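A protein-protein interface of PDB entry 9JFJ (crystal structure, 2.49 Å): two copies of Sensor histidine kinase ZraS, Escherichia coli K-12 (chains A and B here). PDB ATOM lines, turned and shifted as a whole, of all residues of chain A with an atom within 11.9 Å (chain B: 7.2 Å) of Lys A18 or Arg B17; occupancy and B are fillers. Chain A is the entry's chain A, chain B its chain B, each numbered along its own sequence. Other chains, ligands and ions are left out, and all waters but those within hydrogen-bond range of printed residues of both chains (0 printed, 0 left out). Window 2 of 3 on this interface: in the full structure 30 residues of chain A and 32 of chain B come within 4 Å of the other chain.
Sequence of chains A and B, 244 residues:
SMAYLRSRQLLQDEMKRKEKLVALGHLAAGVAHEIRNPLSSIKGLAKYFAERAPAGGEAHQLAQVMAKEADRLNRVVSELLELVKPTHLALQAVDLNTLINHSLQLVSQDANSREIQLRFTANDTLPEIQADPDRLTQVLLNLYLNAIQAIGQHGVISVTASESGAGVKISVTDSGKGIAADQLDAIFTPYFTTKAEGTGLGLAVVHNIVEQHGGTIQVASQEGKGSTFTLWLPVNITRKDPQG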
ATOM      1  N   GLN A   9       2.741 -41.068   7.658  1.00  0.00           N
ATOM      2  CA  GLN A   9       3.242 -41.178   9.044  1.00  0.00           C
ATOM      3  C   GLN A   9       3.905 -39.862   9.454  1.00  0.00           C
ATOM      4  O   GLN A   9       3.781 -39.502  10.623  1.00  0.00           O
ATOM      5  CB  GLN A   9       4.203 -42.358   9.163  1.00  0.00           C
ATOM      6  N   LEU A  10       4.588 -39.189   8.520  1.00  0.00           N
ATOM      7  CA  LEU A  10       5.339 -37.956   8.870  1.00  0.00           C
ATOM      8  C   LEU A  10       4.354 -36.869   9.281  1.00  0.00           C
ATOM      9  O   LEU A  10       4.637 -36.146  10.244  1.00  0.00           O
ATOM     10  CB  LEU A  10       6.156 -37.528   7.651  1.00  0.00           C
ATOM     11  CG  LEU A  10       7.312 -36.575   7.937  1.00  0.00           C
ATOM     12  CD1 LEU A  10       8.261 -37.171   8.962  1.00  0.00           C
ATOM     13  CD2 LEU A  10       8.055 -36.238   6.653  1.00  0.00           C
ATOM     14  N   LEU A  11       3.258 -36.740   8.539  1.00  0.00           N
ATOM     15  CA  LEU A  11       2.207 -35.761   8.906  1.00  0.00           C
ATOM     16  C   LEU A  11       1.601 -36.183  10.245  1.00  0.00           C
ATOM     17  O   LEU A  11       1.458 -35.318  11.120  1.00  0.00           O
ATOM     18  CB  LEU A  11       1.151 -35.746   7.794  1.00  0.00           C
ATOM     19  CG  LEU A  11       0.020 -34.735   7.976  1.00  0.00           C
ATOM     20  CD1 LEU A  11       0.571 -33.329   8.154  1.00  0.00           C
ATOM     21  CD2 LEU A  11      -0.939 -34.781   6.800  1.00  0.00           C
ATOM     22  N   GLN A  12       1.318 -37.473  10.412  1.00  0.00           N
ATOM     23  CA  GLN A  12       0.786 -37.982  11.696  1.00  0.00           C
ATOM     24  C   GLN A  12       1.741 -37.530  12.797  1.00  0.00           C
ATOM     25  O   GLN A  12       1.249 -37.166  13.876  1.00  0.00           O
ATOM     26  CB  GLN A  12       0.699 -39.505  11.639  1.00  0.00           C
ATOM     27  CG  GLN A  12       0.116 -40.150  12.885  1.00  0.00           C
ATOM     28  CD  GLN A  12       0.307 -41.646  12.892  1.00  0.00           C
ATOM     29  OE1 GLN A  12       1.120 -42.196  12.151  1.00  0.00           O
ATOM     30  NE2 GLN A  12      -0.446 -42.324  13.739  1.00  0.00           N
ATOM     31  N   ASP A  13       3.044 -37.496  12.504  1.00  0.00           N
ATOM     32  CA  ASP A  13       4.059 -37.093  13.510  1.00  0.00           C
ATOM     33  C   ASP A  13       3.964 -35.596  13.782  1.00  0.00           C
ATOM     34  O   ASP A  13       3.887 -35.212  14.954  1.00  0.00           O
ATOM     35  CB  ASP A  13       5.478 -37.396  13.032  1.00  0.00           C
ATOM     36  CG  ASP A  13       6.533 -36.522  13.686  1.00  0.00           C
ATOM     37  OD1 ASP A  13       6.669 -36.597  14.922  1.00  0.00           O
ATOM     38  OD2 ASP A  13       7.194 -35.763  12.957  1.00  0.00           O
ATOM     39  N   GLU A  14       4.003 -34.778  12.738  1.00  0.00           N
ATOM     40  CA  GLU A  14       4.021 -33.326  13.024  1.00  0.00           C
ATOM     41  C   GLU A  14       2.737 -33.009  13.775  1.00  0.00           C
ATOM     42  O   GLU A  14       2.757 -32.196  14.744  1.00  0.00           O
ATOM     43  CB  GLU A  14       4.202 -32.509  11.750  1.00  0.00           C
ATOM     44  CG  GLU A  14       4.314 -31.023  12.013  1.00  0.00           C
ATOM     45  N   MET A  15       1.646 -33.700  13.332  1.00  0.00           N
ATOM     46  CA  MET A  15       0.350 -33.387  13.974  1.00  0.00           C
ATOM     47  C   MET A  15       0.448 -33.741  15.455  1.00  0.00           C
ATOM     48  O   MET A  15      -0.110 -33.001  16.270  1.00  0.00           O
ATOM     49  CB  MET A  15      -0.804 -34.145  13.318  1.00  0.00           C
ATOM     50  CG  MET A  15      -1.075 -33.733  11.886  1.00  0.00           C
ATOM     51  SD  MET A  15      -1.509 -31.988  11.702  1.00  0.00           S
ATOM     52  CE  MET A  15      -3.090 -31.945  12.539  1.00  0.00           C
ATOM     53  N   LYS A  16       1.114 -34.794  15.813  1.00  0.00           N
ATOM     54  CA  LYS A  16       1.299 -35.239  17.213  1.00  0.00           C
ATOM     55  C   LYS A  16       2.153 -34.261  18.010  1.00  0.00           C
ATOM     56  O   LYS A  16       1.777 -33.970  19.152  1.00  0.00           O
ATOM     57  CB  LYS A  16       2.038 -36.572  17.211  1.00  0.00           C
ATOM     58  CG  LYS A  16       2.974 -36.792  18.391  1.00  0.00           C
ATOM     59  N   ARG A  17       3.243 -33.756  17.452  1.00  0.00           N
ATOM     60  CA  ARG A  17       3.998 -32.763  18.251  1.00  0.00           C
ATOM     61  C   ARG A  17       3.133 -31.520  18.506  1.00  0.00           C
ATOM     62  O   ARG A  17       3.122 -30.970  19.675  1.00  0.00           O
ATOM     63  CB  ARG A  17       5.346 -32.477  17.589  1.00  0.00           C
ATOM     64  CG  ARG A  17       6.450 -33.454  17.964  1.00  0.00           C
ATOM     65  CD  ARG A  17       6.618 -33.575  19.465  1.00  0.00           C
ATOM     66  NE  ARG A  17       6.503 -32.302  20.164  1.00  0.00           N
ATOM     67  CZ  ARG A  17       6.672 -32.143  21.469  1.00  0.00           C
ATOM     68  NH1 ARG A  17       6.995 -33.179  22.227  1.00  0.00           N
ATOM     69  NH2 ARG A  17       6.536 -30.947  22.013  1.00  0.00           N
ATOM     70  N   LYS A  18       2.414 -31.061  17.499  1.00  0.00           N
ATOM     71  CA  LYS A  18       1.621 -29.834  17.704  1.00  0.00           C
ATOM     72  C   LYS A  18       0.584 -30.141  18.766  1.00  0.00           C
ATOM     73  O   LYS A  18       0.337 -29.289  19.612  1.00  0.00           O
ATOM     74  CB  LYS A  18       0.865 -29.500  16.426  1.00  0.00           C
ATOM     75  CG  LYS A  18       1.723 -29.004  15.274  1.00  0.00           C
ATOM     76  CD  LYS A  18       1.019 -29.067  13.937  1.00  0.00           C
ATOM     77  CE  LYS A  18       1.734 -28.271  12.864  1.00  0.00           C
ATOM     78  NZ  LYS A  18       0.892 -28.109  11.655  1.00  0.00           N
ATOM     79  N   GLU A  19       0.031 -31.340  18.727  1.00  0.00           N
ATOM     80  CA  GLU A  19      -1.050 -31.722  19.651  1.00  0.00           C
ATOM     81  C   GLU A  19      -0.502 -31.710  21.065  1.00  0.00           C
ATOM     82  O   GLU A  19      -1.173 -31.214  21.931  1.00  0.00           O
ATOM     83  CB  GLU A  19      -1.566 -33.100  19.251  1.00  0.00           C
ATOM     84  N   LYS A  20       0.702 -32.228  21.245  1.00  0.00           N
ATOM     85  CA  LYS A  20       1.308 -32.255  22.591  1.00  0.00           C
ATOM     86  C   LYS A  20       1.447 -30.815  23.070  1.00  0.00           C
ATOM     87  O   LYS A  20       0.969 -30.522  24.185  1.00  0.00           O
ATOM     88  CB  LYS A  20       2.624 -33.028  22.570  1.00  0.00           C
ATOM     89  CG  LYS A  20       3.180 -33.404  23.933  1.00  0.00           C
ATOM     90  CD  LYS A  20       4.257 -34.460  23.857  1.00  0.00           C
ATOM     91  N   LEU A  21       1.854 -29.851  22.260  1.00  0.00           N
ATOM     92  CA  LEU A  21       1.993 -28.480  22.837  1.00  0.00           C
ATOM     93  C   LEU A  21       0.638 -27.890  23.246  1.00  0.00           C
ATOM     94  O   LEU A  21       0.521 -27.295  24.367  1.00  0.00           O
ATOM     95  CB  LEU A  21       2.691 -27.570  21.832  1.00  0.00           C
ATOM     96  CG  LEU A  21       3.001 -26.159  22.315  1.00  0.00           C
ATOM     97  CD1 LEU A  21       4.172 -26.177  23.279  1.00  0.00           C
ATOM     98  CD2 LEU A  21       3.298 -25.253  21.135  1.00  0.00           C
ATOM     99  N   VAL A  22      -0.357 -28.015  22.376  1.00  0.00           N
ATOM    100  CA  VAL A  22      -1.691 -27.426  22.664  1.00  0.00           C
ATOM    101  C   VAL A  22      -2.302 -28.099  23.894  1.00  0.00           C
ATOM    102  O   VAL A  22      -2.998 -27.425  24.666  1.00  0.00           O
ATOM    103  CB  VAL A  22      -2.585 -27.483  21.415  1.00  0.00           C
ATOM    104  CG1 VAL A  22      -1.936 -26.800  20.226  1.00  0.00           C
ATOM    105  CG2 VAL A  22      -3.044 -28.886  21.052  1.00  0.00           C
ATOM    106  N   ALA A  23      -2.081 -29.392  24.042  1.00  0.00           N
ATOM    107  CA  ALA A  23      -2.610 -30.138  25.197  1.00  0.00           C
ATOM    108  C   ALA A  23      -1.975 -29.628  26.481  1.00  0.00           C
ATOM    109  O   ALA A  23      -2.668 -29.559  27.495  1.00  0.00           O
ATOM    110  CB  ALA A  23      -2.307 -31.592  25.022  1.00  0.00           C
ATOM    111  N   LEU A  24      -0.677 -29.369  26.435  1.00  0.00           N
ATOM    112  CA  LEU A  24       0.029 -28.858  27.623  1.00  0.00           C
ATOM    113  C   LEU A  24      -0.597 -27.510  27.935  1.00  0.00           C
ATOM    114  O   LEU A  24      -0.930 -27.292  29.090  1.00  0.00           O
ATOM    115  CB  LEU A  24       1.511 -28.721  27.292  1.00  0.00           C
ATOM    116  CG  LEU A  24       2.421 -28.334  28.451  1.00  0.00           C
ATOM    117  CD1 LEU A  24       2.926 -29.571  29.165  1.00  0.00           C
ATOM    118  CD2 LEU A  24       3.582 -27.519  27.932  1.00  0.00           C
ATOM    119  N   GLY A  25      -0.881 -26.720  26.907  1.00  0.00           N
ATOM    120  CA  GLY A  25      -1.572 -25.446  27.177  1.00  0.00           C
ATOM    121  C   GLY A  25      -2.922 -25.618  27.848  1.00  0.00           C
ATOM    122  O   GLY A  25      -3.203 -24.903  28.828  1.00  0.00           O
ATOM    123  N   HIS A  26      -3.679 -26.599  27.385  1.00  0.00           N
ATOM    124  CA  HIS A  26      -5.026 -26.855  27.937  1.00  0.00           C
ATOM    125  C   HIS A  26      -4.911 -27.293  29.394  1.00  0.00           C
ATOM    126  O   HIS A  26      -5.704 -26.830  30.198  1.00  0.00           O
ATOM    127  CB  HIS A  26      -5.738 -27.874  27.047  1.00  0.00           C
ATOM    128  CG  HIS A  26      -6.378 -27.283  25.840  1.00  0.00           C
ATOM    129  ND1 HIS A  26      -6.173 -27.792  24.577  1.00  0.00           N
ATOM    130  CD2 HIS A  26      -7.223 -26.245  25.694  1.00  0.00           C
ATOM    131  CE1 HIS A  26      -6.858 -27.087  23.706  1.00  0.00           C
ATOM    132  NE2 HIS A  26      -7.511 -26.133  24.363  1.00  0.00           N
ATOM    133  N   LEU A  27      -3.950 -28.141  29.691  1.00  0.00           N
ATOM    134  CA  LEU A  27      -3.806 -28.642  31.071  1.00  0.00           C
ATOM    135  C   LEU A  27      -3.353 -27.481  31.961  1.00  0.00           C
ATOM    136  O   LEU A  27      -3.809 -27.411  33.098  1.00  0.00           O
ATOM    137  CB  LEU A  27      -2.813 -29.803  31.072  1.00  0.00           C
ATOM    138  CG  LEU A  27      -3.422 -31.172  30.802  1.00  0.00           C
ATOM    139  CD1 LEU A  27      -2.358 -32.256  30.875  1.00  0.00           C
ATOM    140  CD2 LEU A  27      -4.543 -31.457  31.784  1.00  0.00           C
ATOM    141  N   LEU A  83      -3.037 -16.013  28.723  1.00  0.00           N
ATOM    142  CA  LEU A  83      -1.749 -16.248  28.028  1.00  0.00           C
ATOM    143  C   LEU A  83      -1.457 -17.728  27.755  1.00  0.00           C
ATOM    144  O   LEU A  83      -0.965 -18.009  26.665  1.00  0.00           O
ATOM    145  CB  LEU A  83      -0.641 -15.603  28.861  1.00  0.00           C
ATOM    146  CG  LEU A  83      -0.626 -14.084  28.910  1.00  0.00           C
ATOM    147  CD1 LEU A  83       0.157 -13.598  30.114  1.00  0.00           C
ATOM    148  CD2 LEU A  83      -0.036 -13.516  27.633  1.00  0.00           C
ATOM    149  N   VAL A  84      -1.746 -18.629  28.687  1.00  0.00           N
ATOM    150  CA  VAL A  84      -1.358 -20.059  28.552  1.00  0.00           C
ATOM    151  C   VAL A  84      -2.346 -20.802  27.659  1.00  0.00           C
ATOM    152  O   VAL A  84      -1.994 -21.871  27.149  1.00  0.00           O
ATOM    153  CB  VAL A  84      -1.197 -20.733  29.922  1.00  0.00           C
ATOM    154  CG1 VAL A  84      -0.091 -20.099  30.742  1.00  0.00           C
ATOM    155  CG2 VAL A  84      -2.496 -20.796  30.703  1.00  0.00           C
ATOM    156  N   LYS A  85      -3.512 -20.221  27.458  1.00  0.00           N
ATOM    157  CA  LYS A  85      -4.552 -20.881  26.654  1.00  0.00           C
ATOM    158  C   LYS A  85      -4.055 -21.010  25.220  1.00  0.00           C
ATOM    159  O   LYS A  85      -3.418 -20.071  24.747  1.00  0.00           O
ATOM    160  CB  LYS A  85      -5.891 -20.141  26.700  1.00  0.00           C
ATOM    161  CG  LYS A  85      -6.818 -20.514  27.846  1.00  0.00           C
ATOM    162  CD  LYS A  85      -8.267 -20.591  27.425  1.00  0.00           C
ATOM    163  CE  LYS A  85      -8.724 -19.389  26.631  1.00  0.00           C
ATOM    164  NZ  LYS A  85      -9.990 -19.656  25.907  1.00  0.00           N
ATOM    165  N   PRO A  86      -4.290 -22.135  24.517  1.00  0.00           N
ATOM    166  CA  PRO A  86      -3.919 -22.243  23.105  1.00  0.00           C
ATOM    167  C   PRO A  86      -4.597 -21.162  22.281  1.00  0.00           C
ATOM    168  O   PRO A  86      -5.684 -20.689  22.613  1.00  0.00           O
ATOM    169  CB  PRO A  86      -4.408 -23.636  22.709  1.00  0.00           C
ATOM    170  CG  PRO A  86      -4.447 -24.398  23.976  1.00  0.00           C
ATOM    171  CD  PRO A  86      -4.753 -23.422  25.066  1.00  0.00           C
ATOM    172  N   THR A  87      -3.922 -20.762  21.209  1.00  0.00           N
ATOM    173  CA  THR A  87      -4.461 -19.738  20.325  1.00  0.00           C
ATOM    174  C   THR A  87      -5.807 -20.181  19.766  1.00  0.00           C
ATOM    175  O   THR A  87      -5.918 -21.253  19.167  1.00  0.00           O
ATOM    176  CB  THR A  87      -3.475 -19.455  19.191  1.00  0.00           C
ATOM    177  OG1 THR A  87      -2.245 -18.971  19.740  1.00  0.00           O
ATOM    178  CG2 THR A  87      -4.044 -18.417  18.242  1.00  0.00           C
ATOM    179  N   GLU A 211       0.109 -10.725  18.421  1.00  0.00           N
ATOM    180  CA  GLU A 211       0.914 -11.737  17.748  1.00  0.00           C
ATOM    181  C   GLU A 211       0.024 -12.746  17.046  1.00  0.00           C
ATOM    182  O   GLU A 211       0.261 -13.104  15.887  1.00  0.00           O
ATOM    183  CB  GLU A 211       1.830 -12.428  18.756  1.00  0.00           C
ATOM    184  CG  GLU A 211       2.972 -13.210  18.139  1.00  0.00           C
ATOM    185  CD  GLU A 211       4.175 -13.291  19.052  1.00  0.00           C
ATOM    186  OE1 GLU A 211       4.168 -14.123  19.979  1.00  0.00           O
ATOM    187  OE2 GLU A 211       5.131 -12.516  18.846  1.00  0.00           O
ATOM    188  N   LEU B  10       9.593 -26.895   8.785  1.00  0.00           N
ATOM    189  CA  LEU B  10       8.994 -27.694   9.880  1.00  0.00           C
ATOM    190  C   LEU B  10       9.947 -27.550  11.063  1.00  0.00           C
ATOM    191  O   LEU B  10       9.500 -27.686  12.203  1.00  0.00           O
ATOM    192  CB  LEU B  10       8.898 -29.149   9.417  1.00  0.00           C
ATOM    193  CG  LEU B  10       7.671 -29.914   9.900  1.00  0.00           C
ATOM    194  CD1 LEU B  10       6.407 -29.292   9.335  1.00  0.00           C
ATOM    195  CD2 LEU B  10       7.767 -31.375   9.500  1.00  0.00           C
ATOM    196  N   LEU B  11      11.211 -27.276  10.776  1.00  0.00           N
ATOM    197  CA  LEU B  11      12.244 -27.045  11.812  1.00  0.00           C
ATOM    198  C   LEU B  11      11.900 -25.754  12.538  1.00  0.00           C
ATOM    199  O   LEU B  11      12.080 -25.694  13.759  1.00  0.00           O
ATOM    200  CB  LEU B  11      13.610 -26.908  11.140  1.00  0.00           C
ATOM    201  N   GLN B  12      11.461 -24.755  11.783  1.00  0.00           N
ATOM    202  CA  GLN B  12      11.137 -23.445  12.388  1.00  0.00           C
ATOM    203  C   GLN B  12       9.997 -23.661  13.378  1.00  0.00           C
ATOM    204  O   GLN B  12      10.047 -23.089  14.480  1.00  0.00           O
ATOM    205  CB  GLN B  12      10.737 -22.452  11.301  1.00  0.00           C
ATOM    206  CG  GLN B  12      11.909 -21.686  10.712  1.00  0.00           C
ATOM    207  CD  GLN B  12      12.399 -20.618  11.655  1.00  0.00           C
ATOM    208  OE1 GLN B  12      13.137 -20.884  12.602  1.00  0.00           O
ATOM    209  NE2 GLN B  12      12.000 -19.384  11.400  1.00  0.00           N
ATOM    210  N   ASP B  13       9.018 -24.476  13.002  1.00  0.00           N
ATOM    211  CA  ASP B  13       7.874 -24.758  13.893  1.00  0.00           C
ATOM    212  C   ASP B  13       8.385 -25.436  15.161  1.00  0.00           C
ATOM    213  O   ASP B  13       7.969 -25.026  16.247  1.00  0.00           O
ATOM    214  CB  ASP B  13       6.836 -25.613  13.168  1.00  0.00           C
ATOM    215  CG  ASP B  13       6.083 -24.843  12.100  1.00  0.00           C
ATOM    216  OD1 ASP B  13       6.309 -23.624  11.990  1.00  0.00           O
ATOM    217  OD2 ASP B  13       5.281 -25.470  11.385  1.00  0.00           O
ATOM    218  N   GLU B  14       9.271 -26.411  15.022  1.00  0.00           N
ATOM    219  CA  GLU B  14       9.727 -27.125  16.236  1.00  0.00           C
ATOM    220  C   GLU B  14      10.466 -26.133  17.121  1.00  0.00           C
ATOM    221  O   GLU B  14      10.350 -26.237  18.336  1.00  0.00           O
ATOM    222  CB  GLU B  14      10.581 -28.346  15.914  1.00  0.00           C
ATOM    223  CG  GLU B  14      10.981 -29.155  17.133  1.00  0.00           C
ATOM    224  CD  GLU B  14       9.864 -29.936  17.801  1.00  0.00           C
ATOM    225  OE1 GLU B  14       9.953 -30.163  19.018  1.00  0.00           O
ATOM    226  OE2 GLU B  14       8.921 -30.329  17.098  1.00  0.00           O
ATOM    227  N   MET B  15      11.224 -25.224  16.518  1.00  0.00           N
ATOM    228  CA  MET B  15      11.919 -24.183  17.313  1.00  0.00           C
ATOM    229  C   MET B  15      10.882 -23.368  18.084  1.00  0.00           C
ATOM    230  O   MET B  15      11.045 -23.218  19.301  1.00  0.00           O
ATOM    231  CB  MET B  15      12.674 -23.225  16.390  1.00  0.00           C
ATOM    232  CG  MET B  15      13.941 -23.797  15.808  1.00  0.00           C
ATOM    233  SD  MET B  15      14.823 -22.533  14.874  1.00  0.00           S
ATOM    234  CE  MET B  15      14.499 -21.102  15.899  1.00  0.00           C
ATOM    235  N   LYS B  16       9.865 -22.862  17.393  1.00  0.00           N
ATOM    236  CA  LYS B  16       8.807 -22.021  18.004  1.00  0.00           C
ATOM    237  C   LYS B  16       8.149 -22.756  19.180  1.00  0.00           C
ATOM    238  O   LYS B  16       7.845 -22.099  20.171  1.00  0.00           O
ATOM    239  CB  LYS B  16       7.783 -21.626  16.935  1.00  0.00           C
ATOM    240  N   ARG B  17       7.913 -24.062  19.043  1.00  0.00           N
ATOM    241  CA  ARG B  17       7.280 -24.847  20.121  1.00  0.00           C
ATOM    242  C   ARG B  17       8.199 -24.842  21.328  1.00  0.00           C
ATOM    243  O   ARG B  17       7.707 -24.765  22.466  1.00  0.00           O
ATOM    244  CB  ARG B  17       7.050 -26.285  19.660  1.00  0.00           C
ATOM    245  CG  ARG B  17       5.885 -26.435  18.692  1.00  0.00           C
ATOM    246  CD  ARG B  17       5.510 -27.884  18.458  1.00  0.00           C
ATOM    247  NE  ARG B  17       6.395 -28.531  17.508  1.00  0.00           N
ATOM    248  CZ  ARG B  17       6.263 -28.435  16.197  1.00  0.00           C
ATOM    249  NH1 ARG B  17       5.290 -27.705  15.680  1.00  0.00           N
ATOM    250  NH2 ARG B  17       7.110 -29.057  15.399  1.00  0.00           N
ATOM    251  N   LYS B  18       9.489 -24.985  21.082  1.00  0.00           N
ATOM    252  CA  LYS B  18      10.446 -25.019  22.211  1.00  0.00           C
ATOM    253  C   LYS B  18      10.413 -23.654  22.891  1.00  0.00           C
ATOM    254  O   LYS B  18      10.382 -23.587  24.147  1.00  0.00           O
ATOM    255  CB  LYS B  18      11.818 -25.431  21.681  1.00  0.00           C
ATOM    256  N   GLU B  19      10.331 -22.614  22.080  1.00  0.00           N
ATOM    257  CA  GLU B  19      10.265 -21.255  22.648  1.00  0.00           C
ATOM    258  C   GLU B  19       9.018 -21.140  23.524  1.00  0.00           C
ATOM    259  O   GLU B  19       9.136 -20.592  24.625  1.00  0.00           O
ATOM    260  CB  GLU B  19      10.170 -20.229  21.525  1.00  0.00           C
ATOM    261  CG  GLU B  19      11.503 -19.829  20.937  1.00  0.00           C
ATOM    262  CD  GLU B  19      11.415 -18.638  19.999  1.00  0.00           C
ATOM    263  OE1 GLU B  19      12.043 -17.609  20.298  1.00  0.00           O
ATOM    264  OE2 GLU B  19      10.721 -18.740  18.973  1.00  0.00           O
ATOM    265  N   LYS B  20       7.892 -21.660  23.056  1.00  0.00           N
ATOM    266  CA  LYS B  20       6.625 -21.592  23.824  1.00  0.00           C
ATOM    267  C   LYS B  20       6.726 -22.375  25.129  1.00  0.00           C
ATOM    268  O   LYS B  20       6.253 -21.864  26.142  1.00  0.00           O
ATOM    269  CB  LYS B  20       5.447 -22.065  22.969  1.00  0.00           C
ATOM    270  CG  LYS B  20       4.063 -21.759  23.527  1.00  0.00           C
ATOM    271  CD  LYS B  20       2.961 -21.912  22.507  1.00  0.00           C
ATOM    272  CE  LYS B  20       1.608 -21.478  23.019  1.00  0.00           C
ATOM    273  NZ  LYS B  20       0.550 -21.669  21.994  1.00  0.00           N
ATOM    274  N   LEU B  21       7.356 -23.544  25.113  1.00  0.00           N
ATOM    275  CA  LEU B  21       7.532 -24.290  26.385  1.00  0.00           C
ATOM    276  C   LEU B  21       8.391 -23.468  27.350  1.00  0.00           C
ATOM    277  O   LEU B  21       8.072 -23.438  28.552  1.00  0.00           O
ATOM    278  CB  LEU B  21       8.134 -25.666  26.100  1.00  0.00           C
ATOM    279  CG  LEU B  21       8.452 -26.562  27.302  1.00  0.00           C
ATOM    280  CD1 LEU B  21       7.204 -26.929  28.083  1.00  0.00           C
ATOM    281  CD2 LEU B  21       9.229 -27.798  26.889  1.00  0.00           C
ATOM    282  N   VAL B  22       9.443 -22.834  26.843  1.00  0.00           N
ATOM    283  CA  VAL B  22      10.337 -22.075  27.762  1.00  0.00           C
ATOM    284  C   VAL B  22       9.521 -20.932  28.344  1.00  0.00           C
ATOM    285  O   VAL B  22       9.643 -20.643  29.551  1.00  0.00           O
ATOM    286  CB  VAL B  22      11.621 -21.588  27.064  1.00  0.00           C
ATOM    287  CG1 VAL B  22      12.474 -20.718  27.972  1.00  0.00           C
ATOM    288  CG2 VAL B  22      12.441 -22.753  26.538  1.00  0.00           C
ATOM    289  N   ALA B  23       8.696 -20.333  27.503  1.00  0.00           N
ATOM    290  CA  ALA B  23       7.873 -19.201  27.957  1.00  0.00           C
ATOM    291  C   ALA B  23       6.914 -19.655  29.050  1.00  0.00           C
ATOM    292  O   ALA B  23       6.713 -18.911  30.009  1.00  0.00           O
ATOM    293  CB  ALA B  23       7.125 -18.672  26.782  1.00  0.00           C
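The guanidinium group (NH2) of Arg B17 lies within salt-bridge range of the side-chain carboxylate (OE2) of Glu B14 (2.8 Å).
CG of Glu A14 touches CD1 of Leu B10, 3.8 Å away.
Lys A18 touches Arg B17.
Arg B17 touches Leu A21 (CG to CD2, 3.7 Å).
Lys B20 touches Leu A21 (CD to CD2, 3.6 Å).
Leu A24 touches Leu B21.
Of chain A, only Lys A18 (3.8 Å) and Leu A21 (3.7 Å) come within 4 Å of Arg B17.
Leu B10 touches just one residue of chain A: Glu A14 (3.8 Å).
Glu B14 touches none of the printed residues of chain A.
No residue of chain A comes within 4 Å of Lys B16.
No residue of chain A comes within 4 Å of Lys B18.
No residue of chain A comes within 4 Å of Glu B19.
Lys B20 touches just one residue of chain A: Leu A21 (3.6 Å).
Of chain A, only Leu A24 comes within 4 Å of Leu B21.
Printed residues of chain B within 4 Å of Glu A14: Leu B10.
Of the printed residues of chain B, Leu A24 touches Leu B21 (3.7 Å).
Printed residues of chain B within 4 Å of Leu A21: Arg B17 (3.7 Å) and Lys B20 (3.6 Å).
Glu A19 touches none of the printed residues of chain B.
The nearest residue of chain B that does not touch Lys A18 is Asp B13 (4.8 Å).
The nearest printed residue of chain B that does not touch Leu A21 is Leu B21 (4.5 Å).
Printed residues of chain B that touch a printed residue of chain A: Leu B10, Arg B17, Lys B20 and Leu B21.
Hydrophobic or aromatic side chains of chain B within 4 Å of the printed part of chain A: Leu B10 and Leu B21.
Among the printed residues, 5 pairs touch across the chains.
Glu A14 touches Leu B10, but with the chains exchanged Leu A10 does not touch Glu B14 (10.0 Å).
Lys A18 touches Arg B17, but with the chains exchanged Arg A17 does not touch Lys B18 (6.7 Å).
Leu A21 touches Arg B17, but with the chains exchanged Arg A17 does not touch Leu B21 (6.4 Å).
Leu A21 touches Lys B20, but with the chains exchanged Lys A20 does not touch Leu B21 (8.2 Å).
Positions printed for both chains: 10, 11, 12, 13, 14, 15, 16, 17, 18, 19, 20, 21, 22 and 23.
Of the 5 pairs that touch across the chains among the printed residues, none has its exchanged pair printed and touching as well.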
